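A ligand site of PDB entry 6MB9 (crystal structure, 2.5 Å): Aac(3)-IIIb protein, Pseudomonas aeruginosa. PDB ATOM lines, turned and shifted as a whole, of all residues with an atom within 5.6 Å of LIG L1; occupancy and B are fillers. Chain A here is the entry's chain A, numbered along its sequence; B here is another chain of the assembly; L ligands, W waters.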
ATOM      1  N   VAL A  31     -20.504  12.549   9.254  1.00  0.00           N
ATOM      2  CA  VAL A  31     -20.236  13.884   8.737  1.00  0.00           C
ATOM      3  C   VAL A  31     -19.266  13.794   7.580  1.00  0.00           C
ATOM      4  O   VAL A  31     -18.267  13.060   7.645  1.00  0.00           O
ATOM      5  CB  VAL A  31     -19.716  14.826   9.840  1.00  0.00           C
ATOM      6  CG1 VAL A  31     -18.478  14.251  10.517  1.00  0.00           C
ATOM      7  CG2 VAL A  31     -19.442  16.213   9.275  1.00  0.00           C
ATOM      8  N   HIS A  32     -19.577  14.512   6.489  1.00  0.00           N
ATOM      9  CA  HIS A  32     -18.645  14.772   5.390  1.00  0.00           C
ATOM     10  C   HIS A  32     -18.458  16.282   5.348  1.00  0.00           C
ATOM     11  O   HIS A  32     -19.404  17.019   5.030  1.00  0.00           O
ATOM     12  CB  HIS A  32     -19.191  14.253   4.064  1.00  0.00           C
ATOM     13  CG  HIS A  32     -19.456  12.776   4.057  1.00  0.00           C
ATOM     14  ND1 HIS A  32     -18.465  11.849   3.818  1.00  0.00           N
ATOM     15  CD2 HIS A  32     -20.595  12.072   4.246  1.00  0.00           C
ATOM     16  CE1 HIS A  32     -18.987  10.633   3.876  1.00  0.00           C
ATOM     17  NE2 HIS A  32     -20.272  10.740   4.128  1.00  0.00           N
ATOM     18  N   ALA A  33     -17.253  16.743   5.641  1.00  0.00           N
ATOM     19  CA  ALA A  33     -17.021  18.164   5.883  1.00  0.00           C
ATOM     20  C   ALA A  33     -15.994  18.719   4.902  1.00  0.00           C
ATOM     21  O   ALA A  33     -15.014  18.057   4.560  1.00  0.00           O
ATOM     22  CB  ALA A  33     -16.554  18.408   7.318  1.00  0.00           C
ATOM     23  N   ALA A  34     -16.223  19.949   4.477  1.00  0.00           N
ATOM     24  CA  ALA A  34     -15.240  20.787   3.787  1.00  0.00           C
ATOM     25  C   ALA A  34     -14.879  21.900   4.766  1.00  0.00           C
ATOM     26  O   ALA A  34     -15.517  22.954   4.777  1.00  0.00           O
ATOM     27  CB  ALA A  34     -15.778  21.316   2.457  1.00  0.00           C
ATOM     28  N   VAL A  35     -13.879  21.639   5.609  1.00  0.00           N
ATOM     29  CA  VAL A  35     -13.621  22.510   6.750  1.00  0.00           C
ATOM     30  C   VAL A  35     -13.279  23.930   6.309  1.00  0.00           C
ATOM     31  O   VAL A  35     -13.571  24.902   7.028  1.00  0.00           O
ATOM     32  CB  VAL A  35     -12.508  21.900   7.628  1.00  0.00           C
ATOM     33  CG1 VAL A  35     -12.232  22.771   8.846  1.00  0.00           C
ATOM     34  CG2 VAL A  35     -12.878  20.492   8.057  1.00  0.00           C
ATOM     35  N   SER A  36     -12.706  24.098   5.114  1.00  0.00           N
ATOM     36  CA  SER A  36     -12.344  25.419   4.625  1.00  0.00           C
ATOM     37  C   SER A  36     -13.546  26.334   4.391  1.00  0.00           C
ATOM     38  O   SER A  36     -13.376  27.554   4.360  1.00  0.00           O
ATOM     39  CB  SER A  36     -11.539  25.297   3.331  1.00  0.00           C
ATOM     40  OG  SER A  36     -12.358  24.817   2.276  1.00  0.00           O
ATOM     41  N   ARG A  37     -14.747  25.772   4.228  1.00  0.00           N
ATOM     42  CA  ARG A  37     -15.937  26.576   4.017  1.00  0.00           C
ATOM     43  C   ARG A  37     -16.668  26.935   5.307  1.00  0.00           C
ATOM     44  O   ARG A  37     -17.634  27.694   5.262  1.00  0.00           O
ATOM     45  CB  ARG A  37     -16.916  25.854   3.078  1.00  0.00           C
ATOM     46  CG  ARG A  37     -16.336  25.480   1.728  1.00  0.00           C
ATOM     47  CD  ARG A  37     -17.431  24.980   0.800  1.00  0.00           C
ATOM     48  NE  ARG A  37     -18.370  26.042   0.444  1.00  0.00           N
ATOM     49  CZ  ARG A  37     -19.609  25.824   0.020  1.00  0.00           C
ATOM     50  NH1 ARG A  37     -20.062  24.582  -0.112  1.00  0.00           N
ATOM     51  NH2 ARG A  37     -20.397  26.841  -0.278  1.00  0.00           N
ATOM     52  N   GLY A  44      -9.796  25.012  15.258  1.00  0.00           N
ATOM     53  CA  GLY A  44      -9.640  24.373  13.980  1.00  0.00           C
ATOM     54  C   GLY A  44     -10.672  23.302  13.742  1.00  0.00           C
ATOM     55  O   GLY A  44     -11.821  23.407  14.189  1.00  0.00           O
ATOM     56  N   PRO A  45     -10.294  22.250  13.013  1.00  0.00           N
ATOM     57  CA  PRO A  45     -11.253  21.157  12.733  1.00  0.00           C
ATOM     58  C   PRO A  45     -11.771  20.465  13.975  1.00  0.00           C
ATOM     59  O   PRO A  45     -12.868  19.890  13.931  1.00  0.00           O
ATOM     60  CB  PRO A  45     -10.431  20.196  11.853  1.00  0.00           C
ATOM     61  CG  PRO A  45      -9.386  21.062  11.237  1.00  0.00           C
ATOM     62  CD  PRO A  45      -9.029  22.070  12.284  1.00  0.00           C
ATOM     63  N   TYR A  65     -16.003   8.785   7.316  1.00  0.00           N
ATOM     64  CA  TYR A  65     -15.443   7.799   6.405  1.00  0.00           C
ATOM     65  C   TYR A  65     -13.929   7.941   6.393  1.00  0.00           C
ATOM     66  O   TYR A  65     -13.398   8.988   5.987  1.00  0.00           O
ATOM     67  CB  TYR A  65     -16.018   7.955   5.001  1.00  0.00           C
ATOM     68  CG  TYR A  65     -15.504   6.957   3.994  1.00  0.00           C
ATOM     69  CD1 TYR A  65     -15.396   5.610   4.310  1.00  0.00           C
ATOM     70  CD2 TYR A  65     -15.164   7.348   2.705  1.00  0.00           C
ATOM     71  CE1 TYR A  65     -14.931   4.685   3.388  1.00  0.00           C
ATOM     72  CE2 TYR A  65     -14.692   6.443   1.775  1.00  0.00           C
ATOM     73  CZ  TYR A  65     -14.586   5.112   2.121  1.00  0.00           C
ATOM     74  OH  TYR A  65     -14.127   4.204   1.186  1.00  0.00           O
ATOM     75  N   ASP A 103      -7.913  12.173   0.610  1.00  0.00           N
ATOM     76  CA  ASP A 103      -8.985  12.714  -0.224  1.00  0.00           C
ATOM     77  C   ASP A 103     -10.212  13.076   0.609  1.00  0.00           C
ATOM     78  O   ASP A 103     -10.939  14.016   0.253  1.00  0.00           O
ATOM     79  CB  ASP A 103      -9.366  11.709  -1.304  1.00  0.00           C
ATOM     80  CG  ASP A 103      -8.154  11.154  -2.043  1.00  0.00           C
ATOM     81  OD1 ASP A 103      -8.316  10.158  -2.778  1.00  0.00           O
ATOM     82  OD2 ASP A 103      -7.045  11.699  -1.867  1.00  0.00           O
ATOM     83  N   ASN A 104     -10.446  12.370   1.707  1.00  0.00           N
ATOM     84  CA  ASN A 104     -11.638  12.604   2.525  1.00  0.00           C
ATOM     85  C   ASN A 104     -11.557  13.860   3.361  1.00  0.00           C
ATOM     86  O   ASN A 104     -12.535  14.208   4.025  1.00  0.00           O
ATOM     87  CB  ASN A 104     -11.892  11.405   3.436  1.00  0.00           C
ATOM     88  CG  ASN A 104     -12.330  10.184   2.671  1.00  0.00           C
ATOM     89  OD1 ASN A 104     -12.387  10.192   1.434  1.00  0.00           O
ATOM     90  ND2 ASN A 104     -12.658   9.114   3.387  1.00  0.00           N
ATOM     91  N   GLY A 105     -10.418  14.548   3.370  1.00  0.00           N
ATOM     92  CA  GLY A 105     -10.278  15.789   4.095  1.00  0.00           C
ATOM     93  C   GLY A 105      -9.587  15.587   5.432  1.00  0.00           C
ATOM     94  O   GLY A 105      -9.288  14.475   5.864  1.00  0.00           O
ATOM     95  N   VAL A 106      -9.336  16.716   6.080  1.00  0.00           N
ATOM     96  CA  VAL A 106      -8.629  16.706   7.352  1.00  0.00           C
ATOM     97  C   VAL A 106      -9.483  16.095   8.459  1.00  0.00           C
ATOM     98  O   VAL A 106      -8.953  15.451   9.373  1.00  0.00           O
ATOM     99  CB  VAL A 106      -8.166  18.141   7.690  1.00  0.00           C
ATOM    100  CG1 VAL A 106      -9.365  19.059   7.945  1.00  0.00           C
ATOM    101  CG2 VAL A 106      -7.227  18.138   8.866  1.00  0.00           C
ATOM    102  N   LEU A 107     -10.805  16.266   8.390  1.00  0.00           N
ATOM    103  CA  LEU A 107     -11.666  15.878   9.514  1.00  0.00           C
ATOM    104  C   LEU A 107     -11.628  14.384   9.823  1.00  0.00           C
ATOM    105  O   LEU A 107     -11.478  14.026  11.005  1.00  0.00           O
ATOM    106  CB  LEU A 107     -13.098  16.353   9.266  1.00  0.00           C
ATOM    107  CG  LEU A 107     -13.950  16.387  10.547  1.00  0.00           C
ATOM    108  CD1 LEU A 107     -13.439  17.478  11.492  1.00  0.00           C
ATOM    109  CD2 LEU A 107     -15.424  16.582  10.242  1.00  0.00           C
ATOM    110  N   PRO A 108     -11.792  13.466   8.850  1.00  0.00           N
ATOM    111  CA  PRO A 108     -11.754  12.040   9.212  1.00  0.00           C
ATOM    112  C   PRO A 108     -10.461  11.626   9.906  1.00  0.00           C
ATOM    113  O   PRO A 108     -10.490  10.778  10.799  1.00  0.00           O
ATOM    114  CB  PRO A 108     -11.935  11.330   7.865  1.00  0.00           C
ATOM    115  CG  PRO A 108     -12.666  12.321   7.015  1.00  0.00           C
ATOM    116  CD  PRO A 108     -12.086  13.655   7.418  1.00  0.00           C
ATOM    117  N   PHE A 110      -8.536  13.791  11.706  1.00  0.00           N
ATOM    118  CA  PHE A 110      -8.584  14.425  13.011  1.00  0.00           C
ATOM    119  C   PHE A 110      -9.494  13.655  13.960  1.00  0.00           C
ATOM    120  O   PHE A 110      -9.191  13.518  15.145  1.00  0.00           O
ATOM    121  CB  PHE A 110      -9.069  15.869  12.876  1.00  0.00           C
ATOM    122  CG  PHE A 110      -7.954  16.871  12.785  1.00  0.00           C
ATOM    123  CD1 PHE A 110      -8.003  18.042  13.515  1.00  0.00           C
ATOM    124  CD2 PHE A 110      -6.850  16.626  11.988  1.00  0.00           C
ATOM    125  CE1 PHE A 110      -6.982  18.968  13.435  1.00  0.00           C
ATOM    126  CE2 PHE A 110      -5.820  17.548  11.908  1.00  0.00           C
ATOM    127  CZ  PHE A 110      -5.889  18.727  12.625  1.00  0.00           C
ATOM    128  N   ALA A 168     -19.458  20.046   2.139  1.00  0.00           N
ATOM    129  CA  ALA A 168     -18.819  19.158   1.191  1.00  0.00           C
ATOM    130  C   ALA A 168     -19.714  18.960  -0.039  1.00  0.00           C
ATOM    131  O   ALA A 168     -20.940  19.030   0.065  1.00  0.00           O
ATOM    132  CB  ALA A 168     -18.534  17.799   1.834  1.00  0.00           C
ATOM    133  N   PRO A 169     -19.111  18.736  -1.209  1.00  0.00           N
ATOM    134  CA  PRO A 169     -19.917  18.395  -2.380  1.00  0.00           C
ATOM    135  C   PRO A 169     -20.761  17.162  -2.106  1.00  0.00           C
ATOM    136  O   PRO A 169     -20.315  16.211  -1.474  1.00  0.00           O
ATOM    137  CB  PRO A 169     -18.877  18.140  -3.478  1.00  0.00           C
ATOM    138  CG  PRO A 169     -17.547  18.061  -2.774  1.00  0.00           C
ATOM    139  CD  PRO A 169     -17.681  18.875  -1.534  1.00  0.00           C
ATOM    140  N   ASP A 171     -21.739  14.709  -3.749  1.00  0.00           N
ATOM    141  CA  ASP A 171     -21.355  13.417  -4.310  1.00  0.00           C
ATOM    142  C   ASP A 171     -20.403  12.620  -3.420  1.00  0.00           C
ATOM    143  O   ASP A 171     -20.064  11.489  -3.765  1.00  0.00           O
ATOM    144  CB  ASP A 171     -20.723  13.616  -5.699  1.00  0.00           C
ATOM    145  CG  ASP A 171     -19.481  14.475  -5.663  1.00  0.00           C
ATOM    146  OD1 ASP A 171     -18.380  13.928  -5.414  1.00  0.00           O
ATOM    147  OD2 ASP A 171     -19.594  15.702  -5.871  1.00  0.00           O
ATOM    148  N   THR A 172     -19.968  13.177  -2.290  1.00  0.00           N
ATOM    149  CA  THR A 172     -19.066  12.491  -1.377  1.00  0.00           C
ATOM    150  C   THR A 172     -19.800  11.725  -0.285  1.00  0.00           C
ATOM    151  O   THR A 172     -19.170  11.269   0.671  1.00  0.00           O
ATOM    152  CB  THR A 172     -18.091  13.490  -0.741  1.00  0.00           C
ATOM    153  OG1 THR A 172     -18.822  14.385   0.116  1.00  0.00           O
ATOM    154  CG2 THR A 172     -17.373  14.292  -1.816  1.00  0.00           C
ATOM    155  N   THR A 174     -20.783   8.870   1.393  1.00  0.00           N
ATOM    156  CA  THR A 174     -20.343   7.469   1.327  1.00  0.00           C
ATOM    157  C   THR A 174     -21.507   6.494   1.473  1.00  0.00           C
ATOM    158  O   THR A 174     -21.464   5.407   0.896  1.00  0.00           O
ATOM    159  CB  THR A 174     -19.294   7.195   2.400  1.00  0.00           C
ATOM    160  OG1 THR A 174     -18.271   8.203   2.345  1.00  0.00           O
ATOM    161  CG2 THR A 174     -18.661   5.824   2.193  1.00  0.00           C
ATOM    162  N   GLU B  69      -1.253  24.238  18.224  1.00  0.00           N
ATOM    163  CA  GLU B  69      -2.248  24.938  17.412  1.00  0.00           C
ATOM    164  C   GLU B  69      -3.252  25.622  18.325  1.00  0.00           C
ATOM    165  O   GLU B  69      -4.201  25.000  18.807  1.00  0.00           O
ATOM    166  CB  GLU B  69      -2.910  23.960  16.447  1.00  0.00           C
ATOM    167  CG  GLU B  69      -3.812  24.549  15.368  1.00  0.00           C
ATOM    168  CD  GLU B  69      -3.078  25.405  14.364  1.00  0.00           C
ATOM    169  OE1 GLU B  69      -1.890  25.138  14.099  1.00  0.00           O
ATOM    170  OE2 GLU B  69      -3.725  26.277  13.766  1.00  0.00           O
ATOM    171  N   ALA B 100      -0.495  19.353  16.980  1.00  0.00           N
ATOM    172  CA  ALA B 100       0.721  20.088  16.673  1.00  0.00           C
ATOM    173  C   ALA B 100       0.368  21.278  15.787  1.00  0.00           C
ATOM    174  O   ALA B 100      -0.627  21.254  15.054  1.00  0.00           O
ATOM    175  CB  ALA B 100       1.733  19.186  15.965  1.00  0.00           C
ATOM    176  N   ARG B 102       0.065  23.826  12.855  1.00  0.00           N
ATOM    177  CA  ARG B 102       0.018  23.550  11.429  1.00  0.00           C
ATOM    178  C   ARG B 102       1.231  24.129  10.711  1.00  0.00           C
ATOM    179  O   ARG B 102       1.674  23.579   9.691  1.00  0.00           O
ATOM    180  CB  ARG B 102      -1.276  24.124  10.848  1.00  0.00           C
ATOM    181  CG  ARG B 102      -1.415  23.961   9.348  1.00  0.00           C
ATOM    182  CD  ARG B 102      -2.811  24.362   8.882  1.00  0.00           C
ATOM    183  NE  ARG B 102      -3.067  23.926   7.522  1.00  0.00           N
ATOM    184  CZ  ARG B 102      -3.943  24.517   6.711  1.00  0.00           C
ATOM    185  NH1 ARG B 102      -4.614  25.582   7.137  1.00  0.00           N
ATOM    186  NH2 ARG B 102      -4.128  24.067   5.473  1.00  0.00           N
HETATM  187  N1  LIG L   1      -4.302  22.009  11.314  1.00  0.00           N
HETATM  188  C1  LIG L   1      -5.308  22.912  11.496  1.00  0.00           C
HETATM  189  N2  LIG L   1      -6.234  23.121  10.511  1.00  0.00           N
HETATM  190  C2  LIG L   1      -6.165  22.424   9.351  1.00  0.00           C
HETATM  191  C3  LIG L   1      -5.185  21.539   9.164  1.00  0.00           C
HETATM  192  C4  LIG L   1      -4.233  21.335  10.176  1.00  0.00           C
HETATM  193  N3  LIG L   1      -3.112  20.453  10.205  1.00  0.00           N
HETATM  194  N4  LIG L   1      -5.340  21.000   7.935  1.00  0.00           N
HETATM  195  C5  LIG L   1      -6.415  21.548   7.378  1.00  0.00           C
HETATM  196  N5  LIG L   1      -6.931  22.441   8.240  1.00  0.00           N
HETATM  197  C6  LIG L   1      -8.092  23.278   8.084  1.00  0.00           C
HETATM  198  C7  LIG L   1      -7.799  24.399   7.465  1.00  0.00           C
HETATM  199  O1  LIG L   1      -8.687  25.428   7.921  1.00  0.00           O
HETATM  200  C8  LIG L   1      -8.091  24.123   5.966  1.00  0.00           C
HETATM  201  O2  LIG L   1      -8.460  25.241   5.334  1.00  0.00           O
HETATM  202  P1  LIG L   1      -7.363  26.014   4.285  1.00  0.00           P
HETATM  203  O3  LIG L   1      -8.120  26.909   3.334  1.00  0.00           O
HETATM  204  O4  LIG L   1      -6.575  24.951   3.481  1.00  0.00           O
HETATM  205  O5  LIG L   1      -6.429  26.861   5.118  1.00  0.00           O
HETATM  206  C9  LIG L   1      -9.350  23.193   6.056  1.00  0.00           C
HETATM  207  O6  LIG L   1      -9.219  22.509   7.156  1.00  0.00           O
HETATM  208  C10 LIG L   1      -9.410  22.259   4.869  1.00  0.00           C
HETATM  209  O7  LIG L   1     -10.548  21.471   5.076  1.00  0.00           O
HETATM  210  P2  LIG L   1     -10.621  19.997   4.330  1.00  0.00           P
HETATM  211  O8  LIG L   1      -9.495  19.133   4.807  1.00  0.00           O
HETATM  212  O9  LIG L   1     -11.938  19.356   4.656  1.00  0.00           O
HETATM  213  O10 LIG L   1     -10.514  20.263   2.707  1.00  0.00           O
HETATM  214  P3  LIG L   1     -11.562  21.297   1.861  1.00  0.00           P
HETATM  215  O11 LIG L   1     -10.738  22.215   0.974  1.00  0.00           O
HETATM  216  O12 LIG L   1     -12.382  22.135   2.822  1.00  0.00           O
HETATM  217  O13 LIG L   1     -12.563  20.385   0.932  1.00  0.00           O
HETATM  218  C11 LIG L   1     -12.628  18.078   0.360  1.00  0.00           C
HETATM  219  C12 LIG L   1     -11.936  19.410   0.108  1.00  0.00           C
HETATM  220  C13 LIG L   1     -12.278  17.631   1.742  1.00  0.00           C
HETATM  221  C14 LIG L   1     -12.133  17.057  -0.647  1.00  0.00           C
HETATM  222  C15 LIG L   1     -14.144  18.288   0.229  1.00  0.00           C
HETATM  223  O14 LIG L   1     -14.399  18.779  -1.024  1.00  0.00           O
HETATM  224  C16 LIG L   1     -14.894  16.934   0.413  1.00  0.00           C
HETATM  225  O15 LIG L   1     -15.153  16.237  -0.558  1.00  0.00           O
HETATM  226  N6  LIG L   1     -15.322  16.486   1.806  1.00  0.00           N
HETATM  227  C17 LIG L   1     -16.041  15.150   2.003  1.00  0.00           C
HETATM  228  C18 LIG L   1     -14.943  14.101   2.162  1.00  0.00           C
HETATM  229  C19 LIG L   1     -15.488  12.658   2.249  1.00  0.00           C
HETATM  230  O16 LIG L   1     -16.022  12.256   3.240  1.00  0.00           O
HETATM  231  N7  LIG L   1     -15.302  11.815   1.124  1.00  0.00           N
HETATM  232  C20 LIG L   1     -15.779  10.430   1.116  1.00  0.00           C
HETATM  233  C21 LIG L   1     -15.089   9.729  -0.093  1.00  0.00           C
HETATM  234  S1  LIG L   1     -15.456  10.708  -1.617  1.00  0.00           S
HETATM  235  C1  LG2 L   2     -14.237   8.992  -5.474  1.00  0.00           C
HETATM  236  O1  LG2 L   2     -14.037   8.591  -4.149  1.00  0.00           O
HETATM  237  C2  LG2 L   2     -13.613  10.328  -5.656  1.00  0.00           C
HETATM  238  N1  LG2 L   2     -12.204  10.279  -5.042  1.00  0.00           N
HETATM  239  C3  LG2 L   2     -14.344  11.407  -5.005  1.00  0.00           C
HETATM  240  O2  LG2 L   2     -13.706  12.686  -5.368  1.00  0.00           O
HETATM  241  C4  LG2 L   2     -15.770  11.446  -5.404  1.00  0.00           C
HETATM  242  O3  LG2 L   2     -16.438  12.439  -4.634  1.00  0.00           O
HETATM  243  C5  LG2 L   2     -16.501  10.100  -5.165  1.00  0.00           C
HETATM  244  O4  LG2 L   2     -15.679   8.977  -5.817  1.00  0.00           O
HETATM  245  C6  LG2 L   2     -17.791  10.170  -5.751  1.00  0.00           C
HETATM  246  C7  LG2 L   2     -13.814   4.962  -2.096  1.00  0.00           C
HETATM  247  N2  LG2 L   2     -13.951   3.567  -1.655  1.00  0.00           N
HETATM  248  C8  LG2 L   2     -13.141   4.993  -3.481  1.00  0.00           C
HETATM  249  C9  LG2 L   2     -12.966   6.419  -3.994  1.00  0.00           C
HETATM  250  O5  LG2 L   2     -12.492   6.376  -5.352  1.00  0.00           O
HETATM  251  C10 LG2 L   2     -14.288   7.213  -3.954  1.00  0.00           C
HETATM  252  C11 LG2 L   2     -15.024   7.086  -2.611  1.00  0.00           C
HETATM  253  N3  LG2 L   2     -16.342   7.735  -2.711  1.00  0.00           N
HETATM  254  C12 LG2 L   2     -15.182   5.638  -2.156  1.00  0.00           C
HETATM  255  C13 LG2 L   2     -11.135   6.520  -5.437  1.00  0.00           C
HETATM  256  C14 LG2 L   2     -10.634   5.580  -6.250  1.00  0.00           C
HETATM  257  C15 LG2 L   2     -10.617   6.268  -7.630  1.00  0.00           C
HETATM  258  C16 LG2 L   2     -10.157   7.741  -7.255  1.00  0.00           C
HETATM  259  O6  LG2 L   2     -10.768   7.978  -6.120  1.00  0.00           O
HETATM  260  C17 LG2 L   2     -10.572   8.760  -8.313  1.00  0.00           C
HETATM  261  C18 LG2 L   2     -10.848   5.267 -12.490  1.00  0.00           C
HETATM  262  C19 LG2 L   2     -10.270   4.087 -11.785  1.00  0.00           C
HETATM  263  C20 LG2 L   2      -9.605   4.430 -10.510  1.00  0.00           C
HETATM  264  C21 LG2 L   2     -10.501   5.200  -9.610  1.00  0.00           C
HETATM  265  O7  LG2 L   2      -9.751   5.654  -8.473  1.00  0.00           O
HETATM  266  C22 LG2 L   2     -11.835   6.051 -11.590  1.00  0.00           C
HETATM  267  O8  LG2 L   2     -11.087   6.375 -10.265  1.00  0.00           O
HETATM  268  C23 LG2 L   2     -12.226   7.247 -12.210  1.00  0.00           C
HETATM  269  N4  LG2 L   2     -18.684   9.197  -5.137  1.00  0.00           N
HETATM  270  O9  LG2 L   2      -9.263   5.212  -5.844  1.00  0.00           O
HETATM  271  O10 LG2 L   2     -11.354   3.148 -11.510  1.00  0.00           O
HETATM  272  O11 LG2 L   2      -9.776   6.144 -12.859  1.00  0.00           O
HETATM  273  O12 LG2 L   2     -11.895   9.210  -8.080  1.00  0.00           O
HETATM  274  O13 LG2 L   2     -11.892   4.356  -3.360  1.00  0.00           O
HETATM  275  N5  LG2 L   2     -12.744   8.177 -11.184  1.00  0.00           N
HETATM  276  N6  LG2 L   2      -8.358   5.258 -10.760  1.00  0.00           N
HETATM  277  O   HOH W   1     -17.692   8.165  -0.235  1.00  0.00           O
HETATM  278  O   HOH W   2     -12.754  17.212   6.121  1.00  0.00           O
HETATM  279  O   HOH W   3      -8.653  25.502  10.660  1.00  0.00           O
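Residues that only touch LIG L1: Ala 34 (3.2 Å), Thr 172 (3.2 Å), Pro 169 (3.3 Å), Asp 103 (3.4 Å), Ala 168 (3.5 Å), Pro 45 (3.5 Å), Gly 105 (3.5 Å), Tyr 65 (3.5 Å), Thr 174 (3.6 Å) and Phe 110 (3.9 Å). Hydrophobic or aromatic side chains within 4 Å of LIG L1: His 32, Ala 34, Val 35, Pro 45, Tyr 65, Val 106, Phe 110, Ala 168 and Pro 169. Within 4 Å of LIG L1: His 32, Ala 33, Ala 34, Val 35, Ser 36, Pro 45, Tyr 65, Asp 103, Asn 104, Gly 105, Val 106, Phe 110, Ala 168, Pro 169, Thr 172, Thr 174 and Arg 102 of chain B. The nearest printed residue that does not touch LIG L1 is Glu 69 of chain B (4.4 Å).
ND1 of His 32 sits at hydrogen-bond distance from O16 of LIG L1, at 2.5 Å. An oxygen (O8) of LIG L1 is in hydrogen-bond range of the backbone NH of Val 106. The backbone NH of Ser 36 sits at hydrogen-bond distance from an oxygen (O12) of LIG L1. The side-chain hydroxyl (OG) of Ser 36 is in hydrogen-bond range of an oxygen (O12) of LIG L1 (2.7 Å). NH1 of Arg 102 of chain B lies within salt-bridge range of O5 of LIG L1, 3.0 Å away. OD1 of Asn 104 lies close to N7 of LIG L1, at 3.4 Å. An oxygen (O9) of LIG L1 lies within hydrogen-bond range of the backbone NH of Val 35. A nitrogen (N6) of LIG L1 lies within hydrogen-bond range of the backbone carbonyl oxygen of Ala 33, at 3.2 Å. OH of Tyr 65 lies within hydrogen-bond range of N2 of LG2 L2. The backbone carbonyl oxygen of Asp 171 lies within hydrogen-bond range of a nitrogen (N4) of LG2 L2 (3.0 Å). An oxygen (O3) of LG2 L2 is in hydrogen-bond range of the side-chain carboxylate (OD1) of Asp 171 (2.6 Å).
Water W2 lies within hydrogen-bond range of an oxygen (O9) of LIG L1 (2.7 Å), the backbone carbonyl oxygen (O) of Ala 33 (2.9 Å), the backbone NH (N) of Leu 107 (3.1 Å) and the backbone NH (N) of Val 106 (3.5 Å). Water W1 lies within hydrogen-bond range of the side-chain hydroxyl of Thr 174 (2.6 Å), a nitrogen (N3) of LG2 L2 (2.9 Å) and a sulfur (S1) of LIG L1 (3.7 Å).
ND1 of His 32 lies close to O of Thr 172 (3.3 Å). NE2 of His 32 is in hydrogen-bond range of N of Thr 174. N of Arg 102 of chain B lies within hydrogen-bond range of OE1 of Glu 69 of chain B, at 2.7 Å. The side-chain amide nitrogen (ND2) of Asn 104 sits at hydrogen-bond distance from the backbone carbonyl oxygen (O) of Tyr 65. OG1 of Thr 172 is in hydrogen-bond range of O of Pro 169.
S1 of LIG L1 lies close to N3 of LG2 L2 (3.3 Å).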
